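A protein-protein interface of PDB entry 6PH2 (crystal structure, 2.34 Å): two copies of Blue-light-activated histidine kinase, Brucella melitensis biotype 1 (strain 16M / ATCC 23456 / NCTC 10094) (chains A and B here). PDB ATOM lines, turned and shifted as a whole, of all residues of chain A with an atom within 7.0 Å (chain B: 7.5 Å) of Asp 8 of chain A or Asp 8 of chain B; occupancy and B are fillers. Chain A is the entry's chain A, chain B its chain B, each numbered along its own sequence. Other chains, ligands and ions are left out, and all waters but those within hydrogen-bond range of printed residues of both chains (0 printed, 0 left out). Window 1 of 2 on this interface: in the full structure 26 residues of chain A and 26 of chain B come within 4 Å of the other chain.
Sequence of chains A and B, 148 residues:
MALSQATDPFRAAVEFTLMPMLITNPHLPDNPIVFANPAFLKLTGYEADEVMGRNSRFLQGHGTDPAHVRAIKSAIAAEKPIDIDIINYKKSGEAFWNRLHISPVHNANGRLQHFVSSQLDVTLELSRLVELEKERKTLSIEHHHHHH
Among the printed residues, merely in contact across the chains: Ala 6 of chain A with Gln 113 of chain B, Pro 9 of chain A with His 114 of chain B, Pro 9 of chain A with Val 116 of chain B, Phe 10 of chain A with Arg 11 of chain B, Phe 10 of chain A with Ile 23 of chain B, Arg 11 of chain A with Phe 10 of chain B, Ala 12 of chain A with Val 105 of chain B, Ala 13 of chain A with Val 14 of chain B, Val 105 of chain A with Ala 12 of chain B, Gln 113 of chain A with Ala 6 of chain B, His 114 of chain A with Pro 9 of chain B and Val 116 of chain A with Pro 9 of chain B.
O of Val 105 of chain A lies within hydrogen-bond range of N of Gln 113 of chain A, 2.9 Å away.
O of His 114 of chain A sits at hydrogen-bond distance from N of Val 105 of chain A, at 2.8 Å.
A ring nitrogen (ND1) of His 114 of chain A sits at hydrogen-bond distance from the side-chain amide nitrogen (NE2) of Gln 113 of chain A (2.7 Å).
N of Phe 10 of chain B sits close to OD1 of Asp 8 of chain B (3.4 Å).
The backbone carbonyl oxygen of Val 105 of chain B sits at hydrogen-bond distance from the backbone NH of Gln 113 of chain B, at 2.9 Å.
The backbone NH (N) of Val 105 of chain B lies within hydrogen-bond range of the backbone carbonyl oxygen (O) of His 114 of chain B.
The backbone carbonyl oxygen of Thr 7 of chain A lies within hydrogen-bond range of the side-chain amide nitrogen of Gln 113 of chain B (2.8 Å).
The side-chain amide nitrogen (NE2) of Gln 113 of chain A sits at hydrogen-bond distance from the backbone carbonyl oxygen (O) of Thr 7 of chain B (2.8 Å).
OD2 of Asp 8 of chain A lies close to OD2 of Asp 8 of chain B (3.0 Å).
Of chain A, only Asp 8 (3.0 Å) comes within 4 Å of Asp 8 of chain B.
Of the printed residues of chain A, Val 116 of chain B touches Pro 9 (3.9 Å).
Of the printed residues of chain B, Val 116 of chain A touches Pro 9.
Printed residues of chain A within 4 Å of Val 105 of chain B: Ala 12 (3.7 Å).
Printed residues of chain A within 4 Å of Ala 6 of chain B: Gln 113 (3.7 Å).
Of the printed residues of chain A, Ala 12 of chain B touches Val 105.
Gln 5 of chain A touches none of the printed residues of chain B.
The nearest printed residue of chain A that does not touch Phe 10 of chain B is Phe 10 of chain A (4.01 Å).
Ala 6 of chain A touches Gln 113 of chain B, and with the chains exchanged Gln 113 of chain A touches Ala 6 of chain B.
Thr 7 of chain A touches Gln 113 of chain B, and with the chains exchanged Gln 113 of chain A touches Thr 7 of chain B.
Asp 8 of chain B touches its own counterpart, Asp 8 of chain A.
Phe 10 of chain A touches Arg 11 of chain B, and with the chains exchanged Arg 11 of chain A touches Phe 10 of chain B.
12 positions are printed for both chains.
Of the 15 pairs that touch across the chains among the printed residues, 13 have their exchanged pair printed and touching as well.
Printed residues of chain A that touch a printed residue of chain B: Ala 6, Thr 7, Asp 8, Pro 9, Phe 10, Arg 11, Ala 12, Ala 13, Val 105, Gln 113, His 114 and Val 116.
Hydrophobic or aromatic side chains of chain A within 4 Å of the printed part of chain B: Ala 6, Pro 9, Phe 10, Ala 12, Ala 13, Val 105, His 114 and Val 116.
Of the 14 printed residues of chain B, 13 touch a printed residue of chain A.
Printed residues of chain B that touch a printed residue of chain A: Ala 6, Thr 7, Asp 8, Pro 9, Phe 10, Arg 11, Ala 12, Val 14, Ile 23, Val 105, Gln 113, His 114 and Val 116.
Among the printed residues, no Asp or Glu carboxylate lies within 4 Å of a Lys or Arg side-chain nitrogen of the other chain.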
ATOM      1  N   GLN A   5     -14.854  16.661  24.254  1.00  0.00           N
ATOM      2  CA  GLN A   5     -13.922  15.525  24.314  1.00  0.00           C
ATOM      3  C   GLN A   5     -12.528  16.019  24.742  1.00  0.00           C
ATOM      4  O   GLN A   5     -12.188  17.197  24.578  1.00  0.00           O
ATOM      5  CB  GLN A   5     -13.878  14.801  22.959  1.00  0.00           C
ATOM      6  CG  GLN A   5     -14.122  13.294  23.049  1.00  0.00           C
ATOM      7  CD  GLN A   5     -13.563  12.522  21.874  1.00  0.00           C
ATOM      8  OE1 GLN A   5     -13.927  12.748  20.721  1.00  0.00           O
ATOM      9  NE2 GLN A   5     -12.677  11.581  22.165  1.00  0.00           N
ATOM     10  N   ALA A   6     -11.742  15.109  25.317  1.00  0.00           N
ATOM     11  CA  ALA A   6     -10.290  15.291  25.465  1.00  0.00           C
ATOM     12  C   ALA A   6      -9.683  15.678  24.106  1.00  0.00           C
ATOM     13  O   ALA A   6     -10.060  15.098  23.084  1.00  0.00           O
ATOM     14  CB  ALA A   6      -9.679  14.016  25.994  1.00  0.00           C
ATOM     15  N   THR A   7      -8.785  16.677  24.095  1.00  0.00           N
ATOM     16  CA  THR A   7      -8.164  17.206  22.865  1.00  0.00           C
ATOM     17  C   THR A   7      -7.008  16.312  22.409  1.00  0.00           C
ATOM     18  O   THR A   7      -6.208  15.843  23.228  1.00  0.00           O
ATOM     19  CB  THR A   7      -7.657  18.638  23.067  1.00  0.00           C
ATOM     20  OG1 THR A   7      -8.808  19.397  23.442  1.00  0.00           O
ATOM     21  CG2 THR A   7      -6.999  19.245  21.845  1.00  0.00           C
ATOM     22  N   ASP A   8      -6.935  16.113  21.087  1.00  0.00           N
ATOM     23  CA  ASP A   8      -5.942  15.220  20.460  1.00  0.00           C
ATOM     24  C   ASP A   8      -4.579  15.905  20.583  1.00  0.00           C
ATOM     25  O   ASP A   8      -4.406  17.024  20.089  1.00  0.00           O
ATOM     26  CB  ASP A   8      -6.310  14.907  19.002  1.00  0.00           C
ATOM     27  CG  ASP A   8      -5.349  13.985  18.254  1.00  0.00           C
ATOM     28  OD1 ASP A   8      -4.532  13.291  18.911  1.00  0.00           O
ATOM     29  OD2 ASP A   8      -5.425  13.959  17.004  1.00  0.00           O
ATOM     30  N   PRO A   9      -3.624  15.246  21.274  1.00  0.00           N
ATOM     31  CA  PRO A   9      -2.335  15.872  21.495  1.00  0.00           C
ATOM     32  C   PRO A   9      -1.591  16.080  20.168  1.00  0.00           C
ATOM     33  O   PRO A   9      -0.930  17.115  20.009  1.00  0.00           O
ATOM     34  CB  PRO A   9      -1.584  14.894  22.410  1.00  0.00           C
ATOM     35  CG  PRO A   9      -2.193  13.555  22.085  1.00  0.00           C
ATOM     36  CD  PRO A   9      -3.648  13.890  21.849  1.00  0.00           C
ATOM     37  N   PHE A  10      -1.720  15.132  19.225  1.00  0.00           N
ATOM     38  CA  PHE A  10      -1.006  15.235  17.948  1.00  0.00           C
ATOM     39  C   PHE A  10      -1.562  16.383  17.100  1.00  0.00           C
ATOM     40  O   PHE A  10      -0.792  17.073  16.440  1.00  0.00           O
ATOM     41  CB  PHE A  10      -1.089  13.934  17.171  1.00  0.00           C
ATOM     42  CG  PHE A  10      -0.371  12.787  17.819  1.00  0.00           C
ATOM     43  CD1 PHE A  10       1.000  12.648  17.693  1.00  0.00           C
ATOM     44  CD2 PHE A  10      -1.076  11.840  18.540  1.00  0.00           C
ATOM     45  CE1 PHE A  10       1.660  11.583  18.285  1.00  0.00           C
ATOM     46  CE2 PHE A  10      -0.413  10.768  19.131  1.00  0.00           C
ATOM     47  CZ  PHE A  10       0.955  10.646  19.009  1.00  0.00           C
ATOM     48  N   ARG A  11      -2.879  16.604  17.130  1.00  0.00           N
ATOM     49  CA  ARG A  11      -3.431  17.752  16.418  1.00  0.00           C
ATOM     50  C   ARG A  11      -2.821  19.029  17.007  1.00  0.00           C
ATOM     51  O   ARG A  11      -2.387  19.903  16.265  1.00  0.00           O
ATOM     52  CB  ARG A  11      -4.960  17.769  16.464  1.00  0.00           C
ATOM     53  CG  ARG A  11      -5.592  18.710  15.440  1.00  0.00           C
ATOM     54  CD  ARG A  11      -7.034  19.068  15.735  1.00  0.00           C
ATOM     55  NE  ARG A  11      -7.373  20.395  15.217  1.00  0.00           N
ATOM     56  CZ  ARG A  11      -7.906  20.638  14.018  1.00  0.00           C
ATOM     57  NH1 ARG A  11      -8.274  19.629  13.247  1.00  0.00           N
ATOM     58  NH2 ARG A  11      -8.042  21.882  13.582  1.00  0.00           N
ATOM     59  N   ALA A  12      -2.732  19.109  18.329  1.00  0.00           N
ATOM     60  CA  ALA A  12      -2.200  20.314  19.000  1.00  0.00           C
ATOM     61  C   ALA A  12      -0.703  20.482  18.699  1.00  0.00           C
ATOM     62  O   ALA A  12      -0.212  21.607  18.591  1.00  0.00           O
ATOM     63  CB  ALA A  12      -2.441  20.224  20.480  1.00  0.00           C
ATOM     64  N   ALA A  13       0.017  19.368  18.585  1.00  0.00           N
ATOM     65  CA  ALA A  13       1.417  19.418  18.182  1.00  0.00           C
ATOM     66  C   ALA A  13       1.558  20.185  16.860  1.00  0.00           C
ATOM     67  O   ALA A  13       2.396  21.079  16.743  1.00  0.00           O
ATOM     68  CB  ALA A  13       1.971  18.013  18.051  1.00  0.00           C
ATOM     69  N   VAL A 105       0.340   9.268   3.316  1.00  0.00           N
ATOM     70  CA  VAL A 105      -0.105   8.622   4.545  1.00  0.00           C
ATOM     71  C   VAL A 105      -0.962   7.418   4.159  1.00  0.00           C
ATOM     72  O   VAL A 105      -2.004   7.600   3.562  1.00  0.00           O
ATOM     73  CB  VAL A 105      -0.924   9.581   5.421  1.00  0.00           C
ATOM     74  CG1 VAL A 105      -1.489   8.899   6.648  1.00  0.00           C
ATOM     75  CG2 VAL A 105      -0.121  10.798   5.804  1.00  0.00           C
ATOM     76  N   GLN A 113      -4.384   7.667   1.973  1.00  0.00           N
ATOM     77  CA  GLN A 113      -5.424   8.305   2.773  1.00  0.00           C
ATOM     78  C   GLN A 113      -5.277   9.834   2.719  1.00  0.00           C
ATOM     79  O   GLN A 113      -6.233  10.553   2.480  1.00  0.00           O
ATOM     80  CB  GLN A 113      -5.337   7.812   4.221  1.00  0.00           C
ATOM     81  CG  GLN A 113      -6.635   8.008   5.001  1.00  0.00           C
ATOM     82  CD  GLN A 113      -6.444   7.997   6.499  1.00  0.00           C
ATOM     83  OE1 GLN A 113      -6.464   6.933   7.122  1.00  0.00           O
ATOM     84  NE2 GLN A 113      -6.275   9.181   7.083  1.00  0.00           N
ATOM     85  N   HIS A 114      -4.075  10.322   3.025  1.00  0.00           N
ATOM     86  CA  HIS A 114      -3.763  11.752   3.021  1.00  0.00           C
ATOM     87  C   HIS A 114      -2.346  11.973   2.487  1.00  0.00           C
ATOM     88  O   HIS A 114      -1.580  11.005   2.289  1.00  0.00           O
ATOM     89  CB  HIS A 114      -3.859  12.327   4.434  1.00  0.00           C
ATOM     90  CG  HIS A 114      -5.243  12.462   4.961  1.00  0.00           C
ATOM     91  ND1 HIS A 114      -5.770  11.552   5.856  1.00  0.00           N
ATOM     92  CD2 HIS A 114      -6.181  13.418   4.752  1.00  0.00           C
ATOM     93  CE1 HIS A 114      -7.004  11.937   6.156  1.00  0.00           C
ATOM     94  NE2 HIS A 114      -7.281  13.082   5.480  1.00  0.00           N
ATOM     95  N   VAL A 116       0.831  14.742   3.774  1.00  0.00           N
ATOM     96  CA  VAL A 116       1.246  15.713   4.773  1.00  0.00           C
ATOM     97  C   VAL A 116       2.531  16.364   4.275  1.00  0.00           C
ATOM     98  O   VAL A 116       3.340  15.703   3.613  1.00  0.00           O
ATOM     99  CB  VAL A 116       1.452  15.072   6.163  1.00  0.00           C
ATOM    100  CG1 VAL A 116       0.135  14.615   6.763  1.00  0.00           C
ATOM    101  CG2 VAL A 116       2.460  13.923   6.138  1.00  0.00           C
ATOM    102  N   ALA B   6      -8.233   3.560   9.194  1.00  0.00           N
ATOM    103  CA  ALA B   6      -8.474   4.980   9.630  1.00  0.00           C
ATOM    104  C   ALA B   6      -7.267   5.505  10.430  1.00  0.00           C
ATOM    105  O   ALA B   6      -7.312   5.561  11.660  1.00  0.00           O
ATOM    106  CB  ALA B   6      -9.757   5.048  10.430  1.00  0.00           C
ATOM    107  N   THR B   7      -6.184   5.884   9.739  1.00  0.00           N
ATOM    108  CA  THR B   7      -4.975   6.449  10.386  1.00  0.00           C
ATOM    109  C   THR B   7      -5.165   7.949  10.633  1.00  0.00           C
ATOM    110  O   THR B   7      -5.689   8.657   9.779  1.00  0.00           O
ATOM    111  CB  THR B   7      -3.710   6.277   9.535  1.00  0.00           C
ATOM    112  OG1 THR B   7      -3.632   4.933   9.072  1.00  0.00           O
ATOM    113  CG2 THR B   7      -2.462   6.647  10.301  1.00  0.00           C
ATOM    114  N   ASP B   8      -4.721   8.428  11.794  1.00  0.00           N
ATOM    115  CA  ASP B   8      -4.809   9.851  12.142  1.00  0.00           C
ATOM    116  C   ASP B   8      -3.775  10.616  11.303  1.00  0.00           C
ATOM    117  O   ASP B   8      -2.576  10.332  11.393  1.00  0.00           O
ATOM    118  CB  ASP B   8      -4.630  10.054  13.649  1.00  0.00           C
ATOM    119  CG  ASP B   8      -4.764  11.488  14.132  1.00  0.00           C
ATOM    120  OD1 ASP B   8      -5.317  12.317  13.373  1.00  0.00           O
ATOM    121  OD2 ASP B   8      -4.319  11.756  15.282  1.00  0.00           O
ATOM    122  N   PRO B   9      -4.240  11.564  10.461  1.00  0.00           N
ATOM    123  CA  PRO B   9      -3.303  12.290   9.610  1.00  0.00           C
ATOM    124  C   PRO B   9      -2.342  13.160  10.444  1.00  0.00           C
ATOM    125  O   PRO B   9      -1.163  13.276  10.091  1.00  0.00           O
ATOM    126  CB  PRO B   9      -4.199  13.147   8.705  1.00  0.00           C
ATOM    127  CG  PRO B   9      -5.433  13.379   9.546  1.00  0.00           C
ATOM    128  CD  PRO B   9      -5.612  12.079  10.287  1.00  0.00           C
ATOM    129  N   PHE B  10      -2.836  13.747  11.550  1.00  0.00           N
ATOM    130  CA  PHE B  10      -1.999  14.599  12.390  1.00  0.00           C
ATOM    131  C   PHE B  10      -0.909  13.777  13.092  1.00  0.00           C
ATOM    132  O   PHE B  10       0.211  14.251  13.241  1.00  0.00           O
ATOM    133  CB  PHE B  10      -2.832  15.310  13.449  1.00  0.00           C
ATOM    134  CG  PHE B  10      -3.812  16.302  12.889  1.00  0.00           C
ATOM    135  CD1 PHE B  10      -3.394  17.575  12.552  1.00  0.00           C
ATOM    136  CD2 PHE B  10      -5.145  15.970  12.710  1.00  0.00           C
ATOM    137  CE1 PHE B  10      -4.289  18.504  12.043  1.00  0.00           C
ATOM    138  CE2 PHE B  10      -6.044  16.901  12.209  1.00  0.00           C
ATOM    139  CZ  PHE B  10      -5.615  18.168  11.878  1.00  0.00           C
ATOM    140  N   ARG B  11      -1.219  12.561  13.523  1.00  0.00           N
ATOM    141  CA  ARG B  11      -0.183  11.705  14.100  1.00  0.00           C
ATOM    142  C   ARG B  11       0.899  11.463  13.037  1.00  0.00           C
ATOM    143  O   ARG B  11       2.079  11.559  13.331  1.00  0.00           O
ATOM    144  CB  ARG B  11      -0.747  10.386  14.646  1.00  0.00           C
ATOM    145  CG  ARG B  11       0.201   9.673  15.597  1.00  0.00           C
ATOM    146  CD  ARG B  11      -0.156   8.226  15.840  1.00  0.00           C
ATOM    147  NE  ARG B  11       0.476   7.710  17.047  1.00  0.00           N
ATOM    148  CZ  ARG B  11       1.660   7.093  17.093  1.00  0.00           C
ATOM    149  NH1 ARG B  11       2.352   6.881  15.982  1.00  0.00           N
ATOM    150  NH2 ARG B  11       2.142   6.680  18.256  1.00  0.00           N
ATOM    151  N   ALA B  12       0.497  11.199  11.802  1.00  0.00           N
ATOM    152  CA  ALA B  12       1.450  10.918  10.729  1.00  0.00           C
ATOM    153  C   ALA B  12       2.272  12.173  10.397  1.00  0.00           C
ATOM    154  O   ALA B  12       3.449  12.079  10.041  1.00  0.00           O
ATOM    155  CB  ALA B  12       0.706  10.427   9.517  1.00  0.00           C
ATOM    156  N   ALA B  13       1.657  13.345  10.495  1.00  0.00           N
ATOM    157  CA  ALA B  13       2.387  14.601  10.323  1.00  0.00           C
ATOM    158  C   ALA B  13       3.588  14.649  11.278  1.00  0.00           C
ATOM    159  O   ALA B  13       4.712  14.961  10.880  1.00  0.00           O
ATOM    160  CB  ALA B  13       1.463  15.767  10.547  1.00  0.00           C
ATOM    161  N   VAL B  14       3.340  14.318  12.542  1.00  0.00           N
ATOM    162  CA  VAL B  14       4.355  14.351  13.587  1.00  0.00           C
ATOM    163  C   VAL B  14       5.361  13.209  13.393  1.00  0.00           C
ATOM    164  O   VAL B  14       6.556  13.400  13.594  1.00  0.00           O
ATOM    165  CB  VAL B  14       3.686  14.285  14.968  1.00  0.00           C
ATOM    166  CG1 VAL B  14       4.702  14.112  16.088  1.00  0.00           C
ATOM    167  CG2 VAL B  14       2.797  15.497  15.213  1.00  0.00           C
ATOM    168  N   ILE B  23       5.860  14.937  23.178  1.00  0.00           N
ATOM    169  CA  ILE B  23       4.642  15.183  23.929  1.00  0.00           C
ATOM    170  C   ILE B  23       4.844  14.652  25.348  1.00  0.00           C
ATOM    171  O   ILE B  23       5.336  13.532  25.513  1.00  0.00           O
ATOM    172  CB  ILE B  23       3.436  14.511  23.253  1.00  0.00           C
ATOM    173  CG1 ILE B  23       3.302  14.912  21.789  1.00  0.00           C
ATOM    174  CG2 ILE B  23       2.157  14.817  24.008  1.00  0.00           C
ATOM    175  CD1 ILE B  23       2.317  14.037  21.034  1.00  0.00           C
ATOM    176  N   VAL B 105      -1.251  22.386  26.257  1.00  0.00           N
ATOM    177  CA  VAL B 105      -2.468  22.004  25.560  1.00  0.00           C
ATOM    178  C   VAL B 105      -3.613  21.976  26.571  1.00  0.00           C
ATOM    179  O   VAL B 105      -3.625  21.122  27.438  1.00  0.00           O
ATOM    180  CB  VAL B 105      -2.326  20.632  24.872  1.00  0.00           C
ATOM    181  CG1 VAL B 105      -3.622  20.267  24.167  1.00  0.00           C
ATOM    182  CG2 VAL B 105      -1.144  20.578  23.904  1.00  0.00           C
ATOM    183  N   GLN B 113      -3.772  19.420  29.764  1.00  0.00           N
ATOM    184  CA  GLN B 113      -3.937  18.057  29.302  1.00  0.00           C
ATOM    185  C   GLN B 113      -2.574  17.491  28.894  1.00  0.00           C
ATOM    186  O   GLN B 113      -2.227  16.408  29.317  1.00  0.00           O
ATOM    187  CB  GLN B 113      -4.903  18.039  28.117  1.00  0.00           C
ATOM    188  CG  GLN B 113      -5.542  16.681  27.891  1.00  0.00           C
ATOM    189  CD  GLN B 113      -6.378  16.655  26.640  1.00  0.00           C
ATOM    190  OE1 GLN B 113      -7.009  17.649  26.264  1.00  0.00           O
ATOM    191  NE2 GLN B 113      -6.383  15.502  25.994  1.00  0.00           N
ATOM    192  N   HIS B 114      -1.840  18.219  28.055  1.00  0.00           N
ATOM    193  CA  HIS B 114      -0.523  17.819  27.585  1.00  0.00           C
ATOM    194  C   HIS B 114       0.375  19.054  27.446  1.00  0.00           C
ATOM    195  O   HIS B 114      -0.078  20.198  27.545  1.00  0.00           O
ATOM    196  CB  HIS B 114      -0.608  17.092  26.232  1.00  0.00           C
ATOM    197  CG  HIS B 114      -1.210  15.727  26.290  1.00  0.00           C
ATOM    198  ND1 HIS B 114      -2.550  15.483  25.944  1.00  0.00           N
ATOM    199  CD2 HIS B 114      -0.672  14.530  26.632  1.00  0.00           C
ATOM    200  CE1 HIS B 114      -2.804  14.196  26.084  1.00  0.00           C
ATOM    201  NE2 HIS B 114      -1.660  13.587  26.500  1.00  0.00           N
ATOM    202  N   VAL B 116       3.457  20.040  24.412  1.00  0.00           N
ATOM    203  CA  VAL B 116       4.017  19.629  23.136  1.00  0.00           C
ATOM    204  C   VAL B 116       5.215  20.535  22.867  1.00  0.00           C
ATOM    205  O   VAL B 116       5.212  21.709  23.283  1.00  0.00           O
ATOM    206  CB  VAL B 116       2.988  19.704  21.984  1.00  0.00           C
ATOM    207  CG1 VAL B 116       1.886  18.679  22.140  1.00  0.00           C
ATOM    208  CG2 VAL B 116       2.359  21.081  21.835  1.00  0.00           C
